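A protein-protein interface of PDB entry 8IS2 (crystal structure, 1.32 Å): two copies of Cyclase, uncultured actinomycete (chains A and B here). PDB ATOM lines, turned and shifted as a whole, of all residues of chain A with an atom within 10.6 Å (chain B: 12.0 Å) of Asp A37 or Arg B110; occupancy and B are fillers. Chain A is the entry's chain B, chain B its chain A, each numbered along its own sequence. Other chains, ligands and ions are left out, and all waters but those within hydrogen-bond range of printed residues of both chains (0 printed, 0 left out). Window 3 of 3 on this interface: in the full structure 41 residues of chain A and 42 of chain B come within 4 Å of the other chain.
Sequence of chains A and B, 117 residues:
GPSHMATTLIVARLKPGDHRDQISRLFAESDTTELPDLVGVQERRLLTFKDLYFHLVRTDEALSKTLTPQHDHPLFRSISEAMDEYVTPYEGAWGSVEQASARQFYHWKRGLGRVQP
Of the 10 printed residues of chain B, 5 touch a printed residue of chain A.
Printed residues of chain B that touch a printed residue of chain A: Tyr B106, His B107, Trp B108, Lys B109 and Arg B110.
Hydrophobic or aromatic side chains of chain B that line the printed part of chain A: Tyr B106, His B107 and Trp B108.
Along chain B the printed residues that touch a printed residue of chain A span positions 106 to 110.
Among the printed residues, Asp or Glu carboxylates within 4 Å of a Lys or Arg side-chain nitrogen of the other chain: Asp A37 with Arg B110.
Among the printed residues, merely in contact across the chains: Asp A31 with Trp B108 (3.7 Å), Pro A36 with Trp B108 (3.7 Å), Val A41 with Trp B108 (3.6 Å), Gln A42 with Lys B109 (3.6 Å), Glu A43 with Trp B108 (3.3 Å), Arg A44 with Tyr B106 (3.9 Å), Arg A44 with His B107 (3.4 Å) and Arg A45 with Tyr B106 (3.3 Å).
N of Gln A42 sits at hydrogen-bond distance from O of Arg A58 (2.7 Å).
O of Gly A40 lies within hydrogen-bond range of NE2 of Gln A42, 2.8 Å away.
NH2 of Arg A44 lies within salt-bridge range of OD1 of Asp A31, 2.8 Å away.
O of His B107 is in hydrogen-bond range of N of Val B115 (2.8 Å).
The side-chain carboxylate (OE2) of Glu A43 lies within salt-bridge range of the guanidinium group (NH2) of Arg A45, 2.7 Å away.
The side-chain carboxylate (OE1) of Glu A43 is in salt-bridge range of the guanidinium group (NH1) of Arg A58, at 2.8 Å.
The guanidinium group (NH2) of Arg B110 lies within hydrogen-bond range of the backbone carbonyl oxygen (O) of Pro A36.
OH of Tyr B106 is in hydrogen-bond range of OD2 of Asp A31, 2.4 Å away.
The backbone carbonyl oxygen of Trp B108 sits at hydrogen-bond distance from the backbone NH of Arg A44, 2.9 Å away.
The guanidinium group (NE) of Arg B110 lies within hydrogen-bond range of the backbone carbonyl oxygen (O) of Val A41 (2.9 Å).
The side-chain carboxylate of Asp A37 is in salt-bridge range of the guanidinium group of Arg B110 (3.2 Å).
NE2 of His B107 sits close to NH2 of Arg A45.
N of Arg B110 sits at hydrogen-bond distance from O of Gln A42.
NE2 of His B107 sits at hydrogen-bond distance from OE2 of Glu A43 (2.7 Å).
Of chain B, only Arg B110 (3.2 Å) comes within 4 Å of Asp A37.
Printed residues of chain A within 4 Å of Arg B110: Pro A36 (3.1 Å), Asp A37 (3.2 Å), Val A41 (2.9 Å) and Gln A42 (2.9 Å).
No residue of chain B comes within 4 Å of Leu A35.
Of chain B, only Trp B108 (3.7 Å) and Arg B110 (3.1 Å) come within 4 Å of Pro A36.
No residue of chain B comes within 4 Å of Leu A38.
Of the printed residues of chain B, Glu A43 touches His B107 and Trp B108.
Lys B109 touches just one residue of chain A: Gln A42.
No residue of chain A comes within 4 Å of Gly B111.
Leu B112 touches none of the printed residues of chain A.
No residue of chain A comes within 4 Å of Gly B113.
Of the printed residues of chain B, Asp A31 touches Tyr B106 and Trp B108.
Printed residues of chain B within 4 Å of Gln A42: Lys B109 (3.6 Å) and Arg B110 (2.9 Å).
Of the printed residues of chain A, His B107 touches Glu A43 (2.7 Å), Arg A44 (3.4 Å) and Arg A45 (3.4 Å).
Val A57 touches none of the printed residues of chain B.
Arg A58 touches none of the printed residues of chain B.
The nearest residue of chain B that does not touch Asp A37 is Trp B108 (5.6 Å).
The nearest residue of chain A that does not touch Arg B110 is Gly A40 (4.5 Å).
The nearest printed residue of chain B that does not touch Arg A45 is Trp B108 (5.2 Å).
No position is printed for both chains.
Of the 16 pairs that touch across the chains among the printed residues, none has its exchanged pair printed and touching as well.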
ATOM      1  N   SER A  30     -20.071  18.136  11.455  1.00  0.00           N
ATOM      2  CA  SER A  30     -19.601  16.830  11.898  1.00  0.00           C
ATOM      3  C   SER A  30     -19.047  16.887  13.316  1.00  0.00           C
ATOM      4  O   SER A  30     -19.334  16.006  14.134  1.00  0.00           O
ATOM      5  CB  SER A  30     -18.542  16.306  10.931  1.00  0.00           C
ATOM      6  OG  SER A  30     -17.956  15.115  11.419  1.00  0.00           O
ATOM      7  N   ASP A  31     -18.272  17.926  13.630  1.00  0.00           N
ATOM      8  CA  ASP A  31     -17.587  18.016  14.914  1.00  0.00           C
ATOM      9  C   ASP A  31     -18.511  18.428  16.059  1.00  0.00           C
ATOM     10  O   ASP A  31     -18.062  18.458  17.210  1.00  0.00           O
ATOM     11  CB  ASP A  31     -16.339  18.913  14.795  1.00  0.00           C
ATOM     12  CG  ASP A  31     -15.190  18.224  14.037  1.00  0.00           C
ATOM     13  OD1 ASP A  31     -15.187  16.977  14.002  1.00  0.00           O
ATOM     14  OD2 ASP A  31     -14.278  18.901  13.488  1.00  0.00           O
ATOM     15  N   THR A  32     -19.786  18.734  15.774  1.00  0.00           N
ATOM     16  CA  THR A  32     -20.810  18.869  16.805  1.00  0.00           C
ATOM     17  C   THR A  32     -21.465  17.536  17.154  1.00  0.00           C
ATOM     18  O   THR A  32     -22.119  17.435  18.198  1.00  0.00           O
ATOM     19  CB  THR A  32     -21.891  19.866  16.361  1.00  0.00           C
ATOM     20  OG1 THR A  32     -22.513  19.399  15.163  1.00  0.00           O
ATOM     21  CG2 THR A  32     -21.284  21.231  16.098  1.00  0.00           C
ATOM     22  N   THR A  33     -21.306  16.516  16.314  1.00  0.00           N
ATOM     23  CA  THR A  33     -21.870  15.206  16.594  1.00  0.00           C
ATOM     24  C   THR A  33     -20.966  14.447  17.561  1.00  0.00           C
ATOM     25  O   THR A  33     -19.930  14.944  18.013  1.00  0.00           O
ATOM     26  CB  THR A  33     -22.043  14.403  15.305  1.00  0.00           C
ATOM     27  OG1 THR A  33     -20.770  13.909  14.865  1.00  0.00           O
ATOM     28  CG2 THR A  33     -22.656  15.262  14.206  1.00  0.00           C
ATOM     29  N   GLU A  34     -21.352  13.212  17.870  1.00  0.00           N
ATOM     30  CA  GLU A  34     -20.530  12.365  18.719  1.00  0.00           C
ATOM     31  C   GLU A  34     -19.315  11.804  17.992  1.00  0.00           C
ATOM     32  O   GLU A  34     -18.520  11.093  18.616  1.00  0.00           O
ATOM     33  CB  GLU A  34     -21.368  11.225  19.309  1.00  0.00           C
ATOM     34  CG  GLU A  34     -22.559  11.694  20.145  1.00  0.00           C
ATOM     35  CD  GLU A  34     -22.351  11.502  21.644  1.00  0.00           C
ATOM     36  OE1 GLU A  34     -21.750  10.479  22.039  1.00  0.00           O
ATOM     37  OE2 GLU A  34     -22.788  12.375  22.428  1.00  0.00           O
ATOM     38  N   LEU A  35     -19.148  12.116  16.703  1.00  0.00           N
ATOM     39  CA  LEU A  35     -18.048  11.554  15.918  1.00  0.00           C
ATOM     40  C   LEU A  35     -16.676  11.741  16.555  1.00  0.00           C
ATOM     41  O   LEU A  35     -15.956  10.741  16.703  1.00  0.00           O
ATOM     42  CB  LEU A  35     -18.114  12.044  14.465  1.00  0.00           C
ATOM     43  CG  LEU A  35     -17.047  11.472  13.528  1.00  0.00           C
ATOM     44  CD1 LEU A  35     -17.063   9.954  13.548  1.00  0.00           C
ATOM     45  CD2 LEU A  35     -17.245  11.987  12.111  1.00  0.00           C
ATOM     46  N   PRO A  36     -16.247  12.947  16.948  1.00  0.00           N
ATOM     47  CA  PRO A  36     -14.916  13.058  17.568  1.00  0.00           C
ATOM     48  C   PRO A  36     -14.790  12.281  18.865  1.00  0.00           C
ATOM     49  O   PRO A  36     -13.682  11.855  19.214  1.00  0.00           O
ATOM     50  CB  PRO A  36     -14.722  14.571  17.765  1.00  0.00           C
ATOM     51  CG  PRO A  36     -16.070  15.156  17.657  1.00  0.00           C
ATOM     52  CD  PRO A  36     -16.864  14.271  16.750  1.00  0.00           C
ATOM     53  N   ASP A  37     -15.899  12.057  19.577  1.00  0.00           N
ATOM     54  CA  ASP A  37     -15.851  11.213  20.767  1.00  0.00           C
ATOM     55  C   ASP A  37     -15.646   9.749  20.397  1.00  0.00           C
ATOM     56  O   ASP A  37     -14.935   9.019  21.098  1.00  0.00           O
ATOM     57  CB  ASP A  37     -17.118  11.397  21.600  1.00  0.00           C
ATOM     58  CG  ASP A  37     -17.224  12.790  22.196  1.00  0.00           C
ATOM     59  OD1 ASP A  37     -16.336  13.623  21.915  1.00  0.00           O
ATOM     60  OD2 ASP A  37     -18.188  13.051  22.949  1.00  0.00           O
ATOM     61  N   LEU A  38     -16.252   9.305  19.295  1.00  0.00           N
ATOM     62  CA  LEU A  38     -16.094   7.917  18.873  1.00  0.00           C
ATOM     63  C   LEU A  38     -14.672   7.648  18.397  1.00  0.00           C
ATOM     64  O   LEU A  38     -14.039   6.671  18.818  1.00  0.00           O
ATOM     65  CB  LEU A  38     -17.101   7.592  17.773  1.00  0.00           C
ATOM     66  CG  LEU A  38     -18.549   7.370  18.206  1.00  0.00           C
ATOM     67  CD1 LEU A  38     -19.470   7.498  17.010  1.00  0.00           C
ATOM     68  CD2 LEU A  38     -18.695   6.001  18.837  1.00  0.00           C
ATOM     69  N   VAL A  39     -14.153   8.509  17.519  1.00  0.00           N
ATOM     70  CA  VAL A  39     -12.796   8.340  17.015  1.00  0.00           C
ATOM     71  C   VAL A  39     -11.767   8.607  18.104  1.00  0.00           C
ATOM     72  O   VAL A  39     -10.686   8.004  18.104  1.00  0.00           O
ATOM     73  CB  VAL A  39     -12.572   9.251  15.796  1.00  0.00           C
ATOM     74  CG1 VAL A  39     -11.216   8.966  15.158  1.00  0.00           C
ATOM     75  CG2 VAL A  39     -13.706   9.085  14.796  1.00  0.00           C
ATOM     76  N   GLY A  40     -12.076   9.489  19.050  1.00  0.00           N
ATOM     77  CA  GLY A  40     -11.082   9.922  20.012  1.00  0.00           C
ATOM     78  C   GLY A  40     -10.271  11.106  19.542  1.00  0.00           C
ATOM     79  O   GLY A  40      -9.101  11.241  19.915  1.00  0.00           O
ATOM     80  N   VAL A  41     -10.862  11.970  18.720  1.00  0.00           N
ATOM     81  CA  VAL A  41     -10.137  13.093  18.141  1.00  0.00           C
ATOM     82  C   VAL A  41      -9.791  14.102  19.228  1.00  0.00           C
ATOM     83  O   VAL A  41     -10.660  14.553  19.987  1.00  0.00           O
ATOM     84  CB  VAL A  41     -10.967  13.737  17.018  1.00  0.00           C
ATOM     85  CG1 VAL A  41     -10.280  14.981  16.495  1.00  0.00           C
ATOM     86  CG2 VAL A  41     -11.235  12.753  15.883  1.00  0.00           C
ATOM     87  N   GLN A  42      -8.515  14.457  19.314  1.00  0.00           N
ATOM     88  CA  GLN A  42      -8.091  15.543  20.186  1.00  0.00           C
ATOM     89  C   GLN A  42      -7.992  16.868  19.451  1.00  0.00           C
ATOM     90  O   GLN A  42      -8.235  17.921  20.043  1.00  0.00           O
ATOM     91  CB  GLN A  42      -6.737  15.209  20.819  1.00  0.00           C
ATOM     92  CG  GLN A  42      -6.668  13.814  21.447  1.00  0.00           C
ATOM     93  CD  GLN A  42      -7.713  13.593  22.520  1.00  0.00           C
ATOM     94  OE1 GLN A  42      -7.761  14.323  23.510  1.00  0.00           O
ATOM     95  NE2 GLN A  42      -8.558  12.580  22.332  1.00  0.00           N
ATOM     96  N   GLU A  43      -7.679  16.847  18.160  1.00  0.00           N
ATOM     97  CA  GLU A  43      -7.504  18.077  17.399  1.00  0.00           C
ATOM     98  C   GLU A  43      -7.600  17.755  15.914  1.00  0.00           C
ATOM     99  O   GLU A  43      -7.142  16.696  15.474  1.00  0.00           O
ATOM    100  CB  GLU A  43      -6.132  18.687  17.726  1.00  0.00           C
ATOM    101  CG  GLU A  43      -5.950  20.143  17.335  1.00  0.00           C
ATOM    102  CD  GLU A  43      -4.663  20.738  17.901  1.00  0.00           C
ATOM    103  OE1 GLU A  43      -3.858  19.990  18.498  1.00  0.00           O
ATOM    104  OE2 GLU A  43      -4.456  21.959  17.753  1.00  0.00           O
ATOM    105  N   ARG A  44      -8.183  18.673  15.151  1.00  0.00           N
ATOM    106  CA  ARG A  44      -8.347  18.530  13.707  1.00  0.00           C
ATOM    107  C   ARG A  44      -7.961  19.849  13.059  1.00  0.00           C
ATOM    108  O   ARG A  44      -8.381  20.912  13.531  1.00  0.00           O
ATOM    109  CB  ARG A  44      -9.791  18.164  13.304  1.00  0.00           C
ATOM    110  CG  ARG A  44      -9.962  17.780  11.830  1.00  0.00           C
ATOM    111  CD  ARG A  44     -11.435  17.738  11.373  1.00  0.00           C
ATOM    112  NE  ARG A  44     -12.290  17.045  12.321  1.00  0.00           N
ATOM    113  CZ  ARG A  44     -12.357  15.726  12.447  1.00  0.00           C
ATOM    114  NH1 ARG A  44     -11.610  14.922  11.707  1.00  0.00           N
ATOM    115  NH2 ARG A  44     -13.175  15.200  13.356  1.00  0.00           N
ATOM    116  N   ARG A  45      -7.154  19.781  12.000  1.00  0.00           N
ATOM    117  CA  ARG A  45      -6.780  20.942  11.203  1.00  0.00           C
ATOM    118  C   ARG A  45      -6.984  20.613   9.731  1.00  0.00           C
ATOM    119  O   ARG A  45      -6.542  19.557   9.262  1.00  0.00           O
ATOM    120  CB  ARG A  45      -5.320  21.323  11.448  1.00  0.00           C
ATOM    121  CG  ARG A  45      -5.043  21.846  12.844  1.00  0.00           C
ATOM    122  CD  ARG A  45      -3.563  21.972  13.069  1.00  0.00           C
ATOM    123  NE  ARG A  45      -3.246  22.208  14.471  1.00  0.00           N
ATOM    124  CZ  ARG A  45      -3.076  23.409  15.004  1.00  0.00           C
ATOM    125  NH1 ARG A  45      -3.179  24.508  14.273  1.00  0.00           N
ATOM    126  NH2 ARG A  45      -2.754  23.509  16.292  1.00  0.00           N
ATOM    127  N   VAL A  57      -5.328  15.180  11.649  1.00  0.00           N
ATOM    128  CA  VAL A  57      -6.095  14.782  12.824  1.00  0.00           C
ATOM    129  C   VAL A  57      -5.176  14.127  13.844  1.00  0.00           C
ATOM    130  O   VAL A  57      -4.330  13.298  13.497  1.00  0.00           O
ATOM    131  CB  VAL A  57      -7.291  13.870  12.460  1.00  0.00           C
ATOM    132  CG1 VAL A  57      -6.826  12.541  11.915  1.00  0.00           C
ATOM    133  CG2 VAL A  57      -8.203  13.674  13.657  1.00  0.00           C
ATOM    134  N   ARG A  58      -5.321  14.529  15.102  1.00  0.00           N
ATOM    135  CA  ARG A  58      -4.642  13.904  16.229  1.00  0.00           C
ATOM    136  C   ARG A  58      -5.699  13.190  17.056  1.00  0.00           C
ATOM    137  O   ARG A  58      -6.729  13.783  17.386  1.00  0.00           O
ATOM    138  CB  ARG A  58      -3.945  14.968  17.077  1.00  0.00           C
ATOM    139  CG  ARG A  58      -3.169  14.429  18.269  1.00  0.00           C
ATOM    140  CD  ARG A  58      -2.771  15.552  19.232  1.00  0.00           C
ATOM    141  NE  ARG A  58      -1.487  16.166  18.902  1.00  0.00           N
ATOM    142  CZ  ARG A  58      -1.336  17.248  18.148  1.00  0.00           C
ATOM    143  NH1 ARG A  58      -2.371  17.859  17.596  1.00  0.00           N
ATOM    144  NH2 ARG A  58      -0.114  17.735  17.949  1.00  0.00           N
ATOM    145  N   THR A  59      -5.450  11.924  17.384  1.00  0.00           N
ATOM    146  CA  THR A  59      -6.442  11.115  18.094  1.00  0.00           C
ATOM    147  C   THR A  59      -5.905  10.473  19.378  1.00  0.00           C
ATOM    148  O   THR A  59      -4.790   9.960  19.410  1.00  0.00           O
ATOM    149  CB  THR A  59      -7.030  10.025  17.174  1.00  0.00           C
ATOM    150  OG1 THR A  59      -5.969   9.214  16.654  1.00  0.00           O
ATOM    151  CG2 THR A  59      -7.801  10.657  16.013  1.00  0.00           C
ATOM    152  N   HIS A  73     -19.509   3.320   9.488  1.00  0.00           N
ATOM    153  CA  HIS A  73     -20.297   4.085  10.436  1.00  0.00           C
ATOM    154  C   HIS A  73     -20.909   5.277   9.722  1.00  0.00           C
ATOM    155  O   HIS A  73     -20.202   5.974   8.984  1.00  0.00           O
ATOM    156  CB  HIS A  73     -19.396   4.577  11.571  1.00  0.00           C
ATOM    157  CG  HIS A  73     -20.141   5.178  12.718  1.00  0.00           C
ATOM    158  ND1 HIS A  73     -20.771   6.402  12.637  1.00  0.00           N
ATOM    159  CD2 HIS A  73     -20.353   4.730  13.978  1.00  0.00           C
ATOM    160  CE1 HIS A  73     -21.350   6.673  13.790  1.00  0.00           C
ATOM    161  NE2 HIS A  73     -21.110   5.675  14.623  1.00  0.00           N
ATOM    162  N   LEU A  75     -21.714   8.306  10.522  1.00  0.00           N
ATOM    163  CA  LEU A  75     -21.084   9.605  10.742  1.00  0.00           C
ATOM    164  C   LEU A  75     -19.804   9.738   9.929  1.00  0.00           C
ATOM    165  O   LEU A  75     -19.532  10.800   9.362  1.00  0.00           O
ATOM    166  CB  LEU A  75     -20.804   9.819  12.229  1.00  0.00           C
ATOM    167  CG  LEU A  75     -22.031   9.924  13.137  1.00  0.00           C
ATOM    168  CD1 LEU A  75     -21.646  10.472  14.502  1.00  0.00           C
ATOM    169  CD2 LEU A  75     -23.104  10.780  12.505  1.00  0.00           C
ATOM    170  N   TYR B 106      -9.412  25.629   8.977  1.00  0.00           N
ATOM    171  CA  TYR B 106     -10.311  25.023   9.957  1.00  0.00           C
ATOM    172  C   TYR B 106      -9.465  24.449  11.079  1.00  0.00           C
ATOM    173  O   TYR B 106      -8.474  23.761  10.814  1.00  0.00           O
ATOM    174  CB  TYR B 106     -11.159  23.880   9.355  1.00  0.00           C
ATOM    175  CG  TYR B 106     -12.106  23.179  10.342  1.00  0.00           C
ATOM    176  CD1 TYR B 106     -11.685  22.090  11.100  1.00  0.00           C
ATOM    177  CD2 TYR B 106     -13.428  23.604  10.495  1.00  0.00           C
ATOM    178  CE1 TYR B 106     -12.551  21.446  11.985  1.00  0.00           C
ATOM    179  CE2 TYR B 106     -14.306  22.954  11.371  1.00  0.00           C
ATOM    180  CZ  TYR B 106     -13.863  21.881  12.118  1.00  0.00           C
ATOM    181  OH  TYR B 106     -14.739  21.249  12.986  1.00  0.00           O
ATOM    182  N   HIS B 107      -9.889  24.693  12.319  1.00  0.00           N
ATOM    183  CA  HIS B 107      -9.200  24.175  13.490  1.00  0.00           C
ATOM    184  C   HIS B 107     -10.235  23.852  14.559  1.00  0.00           C
ATOM    185  O   HIS B 107     -10.988  24.725  14.990  1.00  0.00           O
ATOM    186  CB  HIS B 107      -8.197  25.216  13.980  1.00  0.00           C
ATOM    187  CG  HIS B 107      -7.315  24.734  15.076  1.00  0.00           C
ATOM    188  ND1 HIS B 107      -6.494  25.580  15.786  1.00  0.00           N
ATOM    189  CD2 HIS B 107      -7.104  23.494  15.573  1.00  0.00           C
ATOM    190  CE1 HIS B 107      -5.820  24.884  16.685  1.00  0.00           C
ATOM    191  NE2 HIS B 107      -6.170  23.612  16.571  1.00  0.00           N
ATOM    192  N   TRP B 108     -10.291  22.593  14.977  1.00  0.00           N
ATOM    193  CA  TRP B 108     -11.138  22.152  16.078  1.00  0.00           C
ATOM    194  C   TRP B 108     -10.247  21.504  17.129  1.00  0.00           C
ATOM    195  O   TRP B 108      -9.335  20.742  16.795  1.00  0.00           O
ATOM    196  CB  TRP B 108     -12.191  21.141  15.588  1.00  0.00           C
ATOM    197  CG  TRP B 108     -13.111  20.626  16.641  1.00  0.00           C
ATOM    198  CD1 TRP B 108     -14.343  21.116  16.943  1.00  0.00           C
ATOM    199  CD2 TRP B 108     -12.903  19.497  17.506  1.00  0.00           C
ATOM    200  NE1 TRP B 108     -14.913  20.374  17.961  1.00  0.00           N
ATOM    201  CE2 TRP B 108     -14.046  19.376  18.322  1.00  0.00           C
ATOM    202  CE3 TRP B 108     -11.854  18.582  17.677  1.00  0.00           C
ATOM    203  CZ2 TRP B 108     -14.168  18.384  19.295  1.00  0.00           C
ATOM    204  CZ3 TRP B 108     -11.985  17.587  18.651  1.00  0.00           C
ATOM    205  CH2 TRP B 108     -13.128  17.504  19.446  1.00  0.00           C
ATOM    206  N   LYS B 109     -10.515  21.775  18.396  1.00  0.00           N
ATOM    207  CA  LYS B 109      -9.741  21.153  19.449  1.00  0.00           C
ATOM    208  C   LYS B 109     -10.652  20.707  20.583  1.00  0.00           C
ATOM    209  O   LYS B 109     -11.567  21.436  20.982  1.00  0.00           O
ATOM    210  CB  LYS B 109      -8.673  22.108  19.972  1.00  0.00           C
ATOM    211  CG  LYS B 109      -7.755  21.478  20.996  1.00  0.00           C
ATOM    212  CD  LYS B 109      -6.527  22.345  21.275  1.00  0.00           C
ATOM    213  CE  LYS B 109      -5.747  21.829  22.483  1.00  0.00           C
ATOM    214  NZ  LYS B 109      -5.021  22.919  23.196  1.00  0.00           N
ATOM    215  N   ARG B 110     -10.380  19.510  21.106  1.00  0.00           N
ATOM    216  CA  ARG B 110     -11.134  18.979  22.228  1.00  0.00           C
ATOM    217  C   ARG B 110     -11.038  19.936  23.404  1.00  0.00           C
ATOM    218  O   ARG B 110      -9.948  20.374  23.782  1.00  0.00           O
ATOM    219  CB  ARG B 110     -10.585  17.604  22.621  1.00  0.00           C
ATOM    220  CG  ARG B 110     -11.257  16.983  23.836  1.00  0.00           C
ATOM    221  CD  ARG B 110     -10.976  15.488  23.899  1.00  0.00           C
ATOM    222  NE  ARG B 110     -11.507  14.821  22.719  1.00  0.00           N
ATOM    223  CZ  ARG B 110     -12.779  14.481  22.557  1.00  0.00           C
ATOM    224  NH1 ARG B 110     -13.677  14.673  23.512  1.00  0.00           N
ATOM    225  NH2 ARG B 110     -13.160  13.931  21.409  1.00  0.00           N
ATOM    226  N   GLY B 111     -12.188  20.270  23.979  1.00  0.00           N
ATOM    227  CA  GLY B 111     -12.257  21.223  25.060  1.00  0.00           C
ATOM    228  C   GLY B 111     -12.367  22.669  24.635  1.00  0.00           C
ATOM    229  O   GLY B 111     -12.559  23.539  25.500  1.00  0.00           O
ATOM    230  N   LEU B 112     -12.248  22.953  23.343  1.00  0.00           N
ATOM    231  CA  LEU B 112     -12.433  24.292  22.812  1.00  0.00           C
ATOM    232  C   LEU B 112     -13.519  24.368  21.755  1.00  0.00           C
ATOM    233  O   LEU B 112     -14.175  25.410  21.646  1.00  0.00           O
ATOM    234  CB  LEU B 112     -11.123  24.830  22.214  1.00  0.00           C
ATOM    235  CG  LEU B 112      -9.870  24.847  23.093  1.00  0.00           C
ATOM    236  CD1 LEU B 112      -8.691  25.231  22.247  1.00  0.00           C
ATOM    237  CD2 LEU B 112     -10.032  25.828  24.247  1.00  0.00           C
ATOM    238  N   GLY B 113     -13.765  23.286  21.024  1.00  0.00           N
ATOM    239  CA  GLY B 113     -14.608  23.389  19.848  1.00  0.00           C
ATOM    240  C   GLY B 113     -13.842  24.036  18.714  1.00  0.00           C
ATOM    241  O   GLY B 113     -12.628  23.851  18.569  1.00  0.00           O
ATOM    242  N   ARG B 114     -14.538  24.823  17.908  1.00  0.00           N
ATOM    243  CA  ARG B 114     -13.891  25.446  16.764  1.00  0.00           C
ATOM    244  C   ARG B 114     -13.031  26.605  17.239  1.00  0.00           C
ATOM    245  O   ARG B 114     -13.513  27.493  17.948  1.00  0.00           O
ATOM    246  CB  ARG B 114     -14.933  25.935  15.766  1.00  0.00           C
ATOM    247  CG  ARG B 114     -14.341  26.235  14.414  1.00  0.00           C
ATOM    248  CD  ARG B 114     -15.091  27.311  13.673  1.00  0.00           C
ATOM    249  NE  ARG B 114     -14.414  27.613  12.421  1.00  0.00           N
ATOM    250  CZ  ARG B 114     -14.631  26.963  11.287  1.00  0.00           C
ATOM    251  NH1 ARG B 114     -15.514  25.983  11.214  1.00  0.00           N
ATOM    252  NH2 ARG B 114     -13.949  27.308  10.200  1.00  0.00           N
ATOM    253  N   VAL B 115     -11.761  26.591  16.858  1.00  0.00           N
ATOM    254  CA  VAL B 115     -10.842  27.651  17.247  1.00  0.00           C
ATOM    255  C   VAL B 115     -10.898  28.820  16.269  1.00  0.00           C
ATOM    256  O   VAL B 115     -10.824  28.640  15.055  1.00  0.00           O
ATOM    257  CB  VAL B 115      -9.413  27.135  17.414  1.00  0.00           C
ATOM    258  CG1 VAL B 115      -8.496  28.283  17.810  1.00  0.00           C
ATOM    259  CG2 VAL B 115      -9.378  26.028  18.462  1.00  0.00           C
